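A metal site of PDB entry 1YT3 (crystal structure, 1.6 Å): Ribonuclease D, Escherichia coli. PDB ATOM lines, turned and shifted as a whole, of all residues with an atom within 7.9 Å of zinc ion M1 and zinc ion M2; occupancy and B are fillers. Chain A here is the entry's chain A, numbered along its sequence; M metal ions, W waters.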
ATOM      1  N   LEU A  27       7.556  24.302 -21.955  1.00  0.00           N
ATOM      2  CA  LEU A  27       6.357  24.880 -22.549  1.00  0.00           C
ATOM      3  C   LEU A  27       5.387  25.412 -21.504  1.00  0.00           C
ATOM      4  O   LEU A  27       5.399  24.988 -20.344  1.00  0.00           O
ATOM      5  CB  LEU A  27       5.604  23.834 -23.367  1.00  0.00           C
ATOM      6  CG  LEU A  27       6.216  23.202 -24.599  1.00  0.00           C
ATOM      7  CD1 LEU A  27       5.311  22.039 -25.052  1.00  0.00           C
ATOM      8  CD2 LEU A  27       6.341  24.237 -25.707  1.00  0.00           C
ATOM      9  N   ASP A  28       4.537  26.339 -21.928  1.00  0.00           N
ATOM     10  CA  ASP A  28       3.505  26.893 -21.063  1.00  0.00           C
ATOM     11  C   ASP A  28       2.545  27.636 -21.979  1.00  0.00           C
ATOM     12  O   ASP A  28       2.828  27.817 -23.159  1.00  0.00           O
ATOM     13  CB  ASP A  28       4.106  27.852 -20.035  1.00  0.00           C
ATOM     14  CG  ASP A  28       3.092  28.387 -19.054  1.00  0.00           C
ATOM     15  OD1 ASP A  28       2.220  27.596 -18.629  1.00  0.00           O
ATOM     16  OD2 ASP A  28       3.172  29.584 -18.720  1.00  0.00           O
ATOM     17  N   THR A  29       1.376  28.005 -21.457  1.00  0.00           N
ATOM     18  CA  THR A  29       0.405  28.764 -22.235  1.00  0.00           C
ATOM     19  C   THR A  29      -0.259  29.771 -21.321  1.00  0.00           C
ATOM     20  O   THR A  29      -0.154  29.681 -20.102  1.00  0.00           O
ATOM     21  CB  THR A  29      -0.750  27.895 -22.832  1.00  0.00           C
ATOM     22  OG1 THR A  29      -1.575  27.391 -21.769  1.00  0.00           O
ATOM     23  CG2 THR A  29      -0.200  26.728 -23.635  1.00  0.00           C
ATOM     24  N   GLU A  30      -0.919  30.751 -21.919  1.00  0.00           N
ATOM     25  CA  GLU A  30      -1.677  31.732 -21.171  1.00  0.00           C
ATOM     26  C   GLU A  30      -3.020  31.785 -21.888  1.00  0.00           C
ATOM     27  O   GLU A  30      -3.070  31.786 -23.123  1.00  0.00           O
ATOM     28  CB  GLU A  30      -0.998  33.107 -21.194  1.00  0.00           C
ATOM     29  CG  GLU A  30       0.419  33.160 -20.605  1.00  0.00           C
ATOM     30  CD  GLU A  30       0.538  32.616 -19.181  1.00  0.00           C
ATOM     31  OE1 GLU A  30      -0.468  32.594 -18.429  1.00  0.00           O
ATOM     32  OE2 GLU A  30       1.663  32.226 -18.816  1.00  0.00           O
ATOM     33  N   PHE A  31      -4.090  31.779 -21.123  1.00  0.00           N
ATOM     34  CA  PHE A  31      -5.430  31.821 -21.696  1.00  0.00           C
ATOM     35  C   PHE A  31      -6.378  32.469 -20.694  1.00  0.00           C
ATOM     36  O   PHE A  31      -6.072  32.561 -19.509  1.00  0.00           O
ATOM     37  CB  PHE A  31      -5.906  30.409 -22.047  1.00  0.00           C
ATOM     38  CG  PHE A  31      -5.840  29.438 -20.902  1.00  0.00           C
ATOM     39  CD1 PHE A  31      -6.833  29.422 -19.927  1.00  0.00           C
ATOM     40  CD2 PHE A  31      -4.777  28.544 -20.787  1.00  0.00           C
ATOM     41  CE1 PHE A  31      -6.766  28.543 -18.853  1.00  0.00           C
ATOM     42  CE2 PHE A  31      -4.705  27.654 -19.721  1.00  0.00           C
ATOM     43  CZ  PHE A  31      -5.706  27.657 -18.750  1.00  0.00           C
ATOM     44  N   LEU A  43      -1.588  32.952 -25.594  1.00  0.00           N
ATOM     45  CA  LEU A  43      -0.163  32.841 -25.823  1.00  0.00           C
ATOM     46  C   LEU A  43       0.367  31.435 -25.551  1.00  0.00           C
ATOM     47  O   LEU A  43      -0.194  30.694 -24.743  1.00  0.00           O
ATOM     48  CB  LEU A  43       0.567  33.814 -24.888  1.00  0.00           C
ATOM     49  CG  LEU A  43       1.992  34.303 -25.145  1.00  0.00           C
ATOM     50  CD1 LEU A  43       1.998  35.178 -26.405  1.00  0.00           C
ATOM     51  CD2 LEU A  43       2.466  35.105 -23.938  1.00  0.00           C
ATOM     52  N   GLN A  45       4.212  29.655 -24.876  1.00  0.00           N
ATOM     53  CA  GLN A  45       5.613  29.985 -24.622  1.00  0.00           C
ATOM     54  C   GLN A  45       6.487  28.760 -24.768  1.00  0.00           C
ATOM     55  O   GLN A  45       6.098  27.661 -24.360  1.00  0.00           O
ATOM     56  CB  GLN A  45       5.767  30.564 -23.212  1.00  0.00           C
ATOM     57  CG  GLN A  45       4.910  31.795 -22.935  1.00  0.00           C
ATOM     58  CD  GLN A  45       3.632  31.463 -22.190  1.00  0.00           C
ATOM     59  OE1 GLN A  45       2.583  31.247 -22.802  1.00  0.00           O
ATOM     60  NE2 GLN A  45       3.710  31.421 -20.866  1.00  0.00           N
ATOM     61  N   LEU A  79       6.342  20.675 -18.992  1.00  0.00           N
ATOM     62  CA  LEU A  79       5.458  21.723 -18.514  1.00  0.00           C
ATOM     63  C   LEU A  79       5.244  21.475 -17.028  1.00  0.00           C
ATOM     64  O   LEU A  79       5.677  20.440 -16.513  1.00  0.00           O
ATOM     65  CB  LEU A  79       4.124  21.739 -19.276  1.00  0.00           C
ATOM     66  CG  LEU A  79       3.299  20.466 -19.448  1.00  0.00           C
ATOM     67  CD1 LEU A  79       2.828  19.951 -18.103  1.00  0.00           C
ATOM     68  CD2 LEU A  79       2.095  20.770 -20.354  1.00  0.00           C
ATOM     69  N   HIS A  80       4.642  22.433 -16.337  1.00  0.00           N
ATOM     70  CA  HIS A  80       4.362  22.279 -14.917  1.00  0.00           C
ATOM     71  C   HIS A  80       2.871  22.503 -14.696  1.00  0.00           C
ATOM     72  O   HIS A  80       2.344  23.544 -15.098  1.00  0.00           O
ATOM     73  CB  HIS A  80       5.150  23.298 -14.084  1.00  0.00           C
ATOM     74  CG  HIS A  80       4.964  23.131 -12.605  1.00  0.00           C
ATOM     75  ND1 HIS A  80       5.672  22.205 -11.869  1.00  0.00           N
ATOM     76  CD2 HIS A  80       4.116  23.739 -11.741  1.00  0.00           C
ATOM     77  CE1 HIS A  80       5.268  22.246 -10.613  1.00  0.00           C
ATOM     78  NE2 HIS A  80       4.331  23.167 -10.509  1.00  0.00           N
ATOM     79  N   ALA A  81       2.202  21.537 -14.073  1.00  0.00           N
ATOM     80  CA  ALA A  81       0.772  21.609 -13.799  1.00  0.00           C
ATOM     81  C   ALA A  81       0.059  21.882 -15.128  1.00  0.00           C
ATOM     82  O   ALA A  81      -0.609  22.904 -15.286  1.00  0.00           O
ATOM     83  CB  ALA A  81       0.475  22.726 -12.799  1.00  0.00           C
ATOM     84  N   GLY A  82       0.196  20.956 -16.061  1.00  0.00           N
ATOM     85  CA  GLY A  82      -0.380  21.151 -17.380  1.00  0.00           C
ATOM     86  C   GLY A  82      -1.755  20.658 -17.754  1.00  0.00           C
ATOM     87  O   GLY A  82      -2.065  20.620 -18.945  1.00  0.00           O
ATOM     88  N   SER A  83      -2.593  20.278 -16.797  1.00  0.00           N
ATOM     89  CA  SER A  83      -3.922  19.780 -17.127  1.00  0.00           C
ATOM     90  C   SER A  83      -4.656  20.701 -18.107  1.00  0.00           C
ATOM     91  O   SER A  83      -5.148  20.251 -19.144  1.00  0.00           O
ATOM     92  CB  SER A  83      -4.782  19.591 -15.870  1.00  0.00           C
ATOM     93  OG  SER A  83      -6.057  19.073 -16.204  1.00  0.00           O
ATOM     94  N   GLU A  84      -4.722  21.993 -17.795  1.00  0.00           N
ATOM     95  CA  GLU A  84      -5.400  22.932 -18.682  1.00  0.00           C
ATOM     96  C   GLU A  84      -4.615  23.161 -19.959  1.00  0.00           C
ATOM     97  O   GLU A  84      -5.197  23.403 -21.021  1.00  0.00           O
ATOM     98  CB  GLU A  84      -5.655  24.251 -17.964  1.00  0.00           C
ATOM     99  CG  GLU A  84      -6.649  24.116 -16.815  1.00  0.00           C
ATOM    100  CD  GLU A  84      -6.998  25.452 -16.197  1.00  0.00           C
ATOM    101  OE1 GLU A  84      -6.116  26.081 -15.584  1.00  0.00           O
ATOM    102  OE2 GLU A  84      -8.172  25.864 -16.335  1.00  0.00           O
ATOM    103  N   ASP A  85      -3.286  23.096 -19.868  1.00  0.00           N
ATOM    104  CA  ASP A  85      -2.463  23.289 -21.057  1.00  0.00           C
ATOM    105  C   ASP A  85      -2.781  22.179 -22.056  1.00  0.00           C
ATOM    106  O   ASP A  85      -2.835  22.418 -23.259  1.00  0.00           O
ATOM    107  CB  ASP A  85      -0.974  23.227 -20.712  1.00  0.00           C
ATOM    108  CG  ASP A  85      -0.534  24.340 -19.785  1.00  0.00           C
ATOM    109  OD1 ASP A  85      -0.807  25.517 -20.092  1.00  0.00           O
ATOM    110  OD2 ASP A  85       0.094  24.026 -18.751  1.00  0.00           O
ATOM    111  N   LEU A  86      -2.985  20.970 -21.551  1.00  0.00           N
ATOM    112  CA  LEU A  86      -3.303  19.855 -22.437  1.00  0.00           C
ATOM    113  C   LEU A  86      -4.595  20.149 -23.198  1.00  0.00           C
ATOM    114  O   LEU A  86      -4.686  19.890 -24.397  1.00  0.00           O
ATOM    115  CB  LEU A  86      -3.452  18.561 -21.635  1.00  0.00           C
ATOM    116  CG  LEU A  86      -2.202  18.100 -20.880  1.00  0.00           C
ATOM    117  CD1 LEU A  86      -2.496  16.791 -20.168  1.00  0.00           C
ATOM    118  CD2 LEU A  86      -1.045  17.938 -21.851  1.00  0.00           C
ATOM    119  N   VAL A  88      -5.868  23.094 -23.966  1.00  0.00           N
ATOM    120  CA  VAL A  88      -5.602  24.109 -24.980  1.00  0.00           C
ATOM    121  C   VAL A  88      -4.850  23.529 -26.167  1.00  0.00           C
ATOM    122  O   VAL A  88      -5.146  23.851 -27.317  1.00  0.00           O
ATOM    123  CB  VAL A  88      -4.816  25.326 -24.391  1.00  0.00           C
ATOM    124  CG1 VAL A  88      -5.449  25.769 -23.078  1.00  0.00           C
ATOM    125  CG2 VAL A  88      -3.354  24.982 -24.197  1.00  0.00           C
ATOM    126  N   PHE A  89      -3.871  22.662 -25.901  1.00  0.00           N
ATOM    127  CA  PHE A  89      -3.102  22.042 -26.962  1.00  0.00           C
ATOM    128  C   PHE A  89      -4.007  21.223 -27.878  1.00  0.00           C
ATOM    129  O   PHE A  89      -3.891  21.295 -29.098  1.00  0.00           O
ATOM    130  CB  PHE A  89      -2.014  21.120 -26.378  1.00  0.00           C
ATOM    131  CG  PHE A  89      -0.873  21.854 -25.736  1.00  0.00           C
ATOM    132  CD1 PHE A  89      -0.104  21.230 -24.757  1.00  0.00           C
ATOM    133  CD2 PHE A  89      -0.532  23.145 -26.129  1.00  0.00           C
ATOM    134  CE1 PHE A  89       0.973  21.892 -24.173  1.00  0.00           C
ATOM    135  CE2 PHE A  89       0.550  23.820 -25.546  1.00  0.00           C
ATOM    136  CZ  PHE A  89       1.305  23.178 -24.566  1.00  0.00           C
ATOM    137  N   PHE A 118       4.082  26.469  -9.209  1.00  0.00           N
ATOM    138  CA  PHE A 118       5.247  26.832  -9.987  1.00  0.00           C
ATOM    139  C   PHE A 118       6.149  27.803  -9.240  1.00  0.00           C
ATOM    140  O   PHE A 118       7.360  27.592  -9.151  1.00  0.00           O
ATOM    141  CB  PHE A 118       4.834  27.450 -11.321  1.00  0.00           C
ATOM    142  CG  PHE A 118       5.981  27.787 -12.219  1.00  0.00           C
ATOM    143  CD1 PHE A 118       6.756  26.785 -12.791  1.00  0.00           C
ATOM    144  CD2 PHE A 118       6.320  29.120 -12.476  1.00  0.00           C
ATOM    145  CE1 PHE A 118       7.842  27.082 -13.608  1.00  0.00           C
ATOM    146  CE2 PHE A 118       7.410  29.430 -13.294  1.00  0.00           C
ATOM    147  CZ  PHE A 118       8.171  28.411 -13.855  1.00  0.00           C
ATOM    148  N   SER A 135      -0.095  37.687 -13.267  1.00  0.00           N
ATOM    149  CA  SER A 135      -0.713  36.375 -13.388  1.00  0.00           C
ATOM    150  C   SER A 135      -2.168  36.420 -13.870  1.00  0.00           C
ATOM    151  O   SER A 135      -2.537  35.711 -14.797  1.00  0.00           O
ATOM    152  CB  SER A 135      -0.656  35.642 -12.048  1.00  0.00           C
ATOM    153  OG  SER A 135      -1.272  34.371 -12.133  1.00  0.00           O
ATOM    154  N   TRP A 139      -4.965  38.141 -21.210  1.00  0.00           N
ATOM    155  CA  TRP A 139      -4.049  37.603 -22.197  1.00  0.00           C
ATOM    156  C   TRP A 139      -4.480  37.758 -23.652  1.00  0.00           C
ATOM    157  O   TRP A 139      -3.743  37.403 -24.563  1.00  0.00           O
ATOM    158  CB  TRP A 139      -3.757  36.134 -21.886  1.00  0.00           C
ATOM    159  CG  TRP A 139      -2.999  35.999 -20.600  1.00  0.00           C
ATOM    160  CD1 TRP A 139      -3.474  35.570 -19.407  1.00  0.00           C
ATOM    161  CD2 TRP A 139      -1.635  36.385 -20.376  1.00  0.00           C
ATOM    162  NE1 TRP A 139      -2.505  35.656 -18.442  1.00  0.00           N
ATOM    163  CE2 TRP A 139      -1.364  36.150 -19.015  1.00  0.00           C
ATOM    164  CE3 TRP A 139      -0.623  36.904 -21.194  1.00  0.00           C
ATOM    165  CZ2 TRP A 139      -0.114  36.434 -18.445  1.00  0.00           C
ATOM    166  CZ3 TRP A 139       0.619  37.182 -20.634  1.00  0.00           C
ATOM    167  CH2 TRP A 139       0.862  36.935 -19.264  1.00  0.00           C
ATOM    168  N   TYR A 151       6.305  38.074 -17.546  1.00  0.00           N
ATOM    169  CA  TYR A 151       5.684  37.065 -16.692  1.00  0.00           C
ATOM    170  C   TYR A 151       5.562  35.769 -17.472  1.00  0.00           C
ATOM    171  O   TYR A 151       5.935  34.700 -16.988  1.00  0.00           O
ATOM    172  CB  TYR A 151       4.290  37.516 -16.246  1.00  0.00           C
ATOM    173  CG  TYR A 151       3.493  36.400 -15.616  1.00  0.00           C
ATOM    174  CD1 TYR A 151       3.647  36.085 -14.266  1.00  0.00           C
ATOM    175  CD2 TYR A 151       2.621  35.619 -16.382  1.00  0.00           C
ATOM    176  CE1 TYR A 151       2.954  35.011 -13.693  1.00  0.00           C
ATOM    177  CE2 TYR A 151       1.929  34.543 -15.819  1.00  0.00           C
ATOM    178  CZ  TYR A 151       2.107  34.250 -14.480  1.00  0.00           C
ATOM    179  OH  TYR A 151       1.433  33.181 -13.926  1.00  0.00           O
ATOM    180  N   ALA A 152       5.014  35.859 -18.686  1.00  0.00           N
ATOM    181  CA  ALA A 152       4.831  34.691 -19.536  1.00  0.00           C
ATOM    182  C   ALA A 152       6.159  34.005 -19.849  1.00  0.00           C
ATOM    183  O   ALA A 152       6.242  32.777 -19.864  1.00  0.00           O
ATOM    184  CB  ALA A 152       4.135  35.090 -20.827  1.00  0.00           C
ATOM    185  N   ALA A 153       7.188  34.808 -20.102  1.00  0.00           N
ATOM    186  CA  ALA A 153       8.510  34.273 -20.433  1.00  0.00           C
ATOM    187  C   ALA A 153       9.121  33.549 -19.243  1.00  0.00           C
ATOM    188  O   ALA A 153       9.747  32.493 -19.397  1.00  0.00           O
ATOM    189  CB  ALA A 153       9.422  35.394 -20.873  1.00  0.00           C
ATOM    190  N   ALA A 154       8.956  34.109 -18.047  1.00  0.00           N
ATOM    191  CA  ALA A 154       9.510  33.505 -16.845  1.00  0.00           C
ATOM    192  C   ALA A 154       8.981  32.104 -16.585  1.00  0.00           C
ATOM    193  O   ALA A 154       9.686  31.264 -16.011  1.00  0.00           O
ATOM    194  CB  ALA A 154       9.239  34.398 -15.635  1.00  0.00           C
ATOM    195  N   ASP A 155       7.752  31.840 -17.015  1.00  0.00           N
ATOM    196  CA  ASP A 155       7.149  30.529 -16.811  1.00  0.00           C
ATOM    197  C   ASP A 155       7.855  29.402 -17.546  1.00  0.00           C
ATOM    198  O   ASP A 155       7.672  28.224 -17.204  1.00  0.00           O
ATOM    199  CB  ASP A 155       5.660  30.567 -17.164  1.00  0.00           C
ATOM    200  CG  ASP A 155       4.815  31.159 -16.046  1.00  0.00           C
ATOM    201  OD1 ASP A 155       5.371  31.498 -14.981  1.00  0.00           O
ATOM    202  OD2 ASP A 155       3.592  31.284 -16.226  1.00  0.00           O
ATOM    203  N   VAL A 156       8.644  29.726 -18.572  1.00  0.00           N
ATOM    204  CA  VAL A 156       9.396  28.686 -19.252  1.00  0.00           C
ATOM    205  C   VAL A 156      10.895  28.860 -19.014  1.00  0.00           C
ATOM    206  O   VAL A 156      11.646  27.881 -18.985  1.00  0.00           O
ATOM    207  CB  VAL A 156       9.109  28.640 -20.784  1.00  0.00           C
ATOM    208  CG1 VAL A 156       7.690  28.138 -21.009  1.00  0.00           C
ATOM    209  CG2 VAL A 156       9.303  29.992 -21.417  1.00  0.00           C
HETATM  210 ZN    ZN M   1       2.311  30.729 -17.454  1.00  0.00          ZN
HETATM  211 ZN    ZN M   2       0.387  25.996 -17.832  1.00  0.00          ZN
HETATM  212  O   HOH W   1      -0.931  27.618 -18.322  1.00  0.00           O
HETATM  213  O   HOH W   2       0.958  29.583 -16.662  1.00  0.00           O
HETATM  214  O   HOH W   3      -0.302  25.610 -15.025  1.00  0.00           O
HETATM  215  O   HOH W   4       1.734  25.240 -17.045  1.00  0.00           O
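Water W1 lies within hydrogen-bond range of the side-chain carboxylate of Asp 85 (2.7 Å) and the backbone carbonyl oxygen of Thr 29 (2.8 Å).
Merely in contact with zinc ion M1: Gln 45 (3.8 Å) and Thr 29 (3.8 Å). Within 4 Å of zinc ion M1: Asp 28, Thr 29, Glu 30, Gln 45 and Asp 155. The nearest printed residue that does not touch zinc ion M1 is Tyr 151 (4.2 Å).
Zinc ion M2 is bound by water W4 (1.7 Å), water W1 (2.1 Å), the side-chain carboxylate (OD2) of Asp 85 (2.2 Å) and the side-chain carboxylate (OD1) of Asp 28 (2.6 Å). Slightly farther from zinc ion M2 lies OD1 of Asp 85 (2.6 Å).
The backbone NH (N) of Gln 45 sits at hydrogen-bond distance from the backbone carbonyl oxygen (O) of Asp 28, 2.9 Å away. The side-chain carboxylate (OE2) of Glu 30 sits close to the side-chain amide nitrogen (NE2) of Gln 45 (3.0 Å). The backbone carbonyl oxygen (O) of Leu 43 sits at hydrogen-bond distance from the backbone NH (N) of Glu 30 (2.9 Å). OG1 of Thr 29 lies within hydrogen-bond range of OD1 of Asp 85 (2.6 Å). The side-chain amide nitrogen (NE2) of Gln 45 is in hydrogen-bond range of the backbone carbonyl oxygen (O) of Ala 152 (3.0 Å). The backbone carbonyl oxygen of Leu 43 lies close to the side-chain amide oxygen of Gln 45 (3.4 Å).
Within 4 Å of zinc ion M2: Asp 28 and Asp 85. The nearest printed residue that does not touch zinc ion M2 is Ala 81 (4.1 Å).
Zinc ion M1 is bound by OD2 of Asp 155, OD2 of Asp 28, water W2 and OE2 of Glu 30. Zinc ion M1 has four donor atoms within binding distance.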
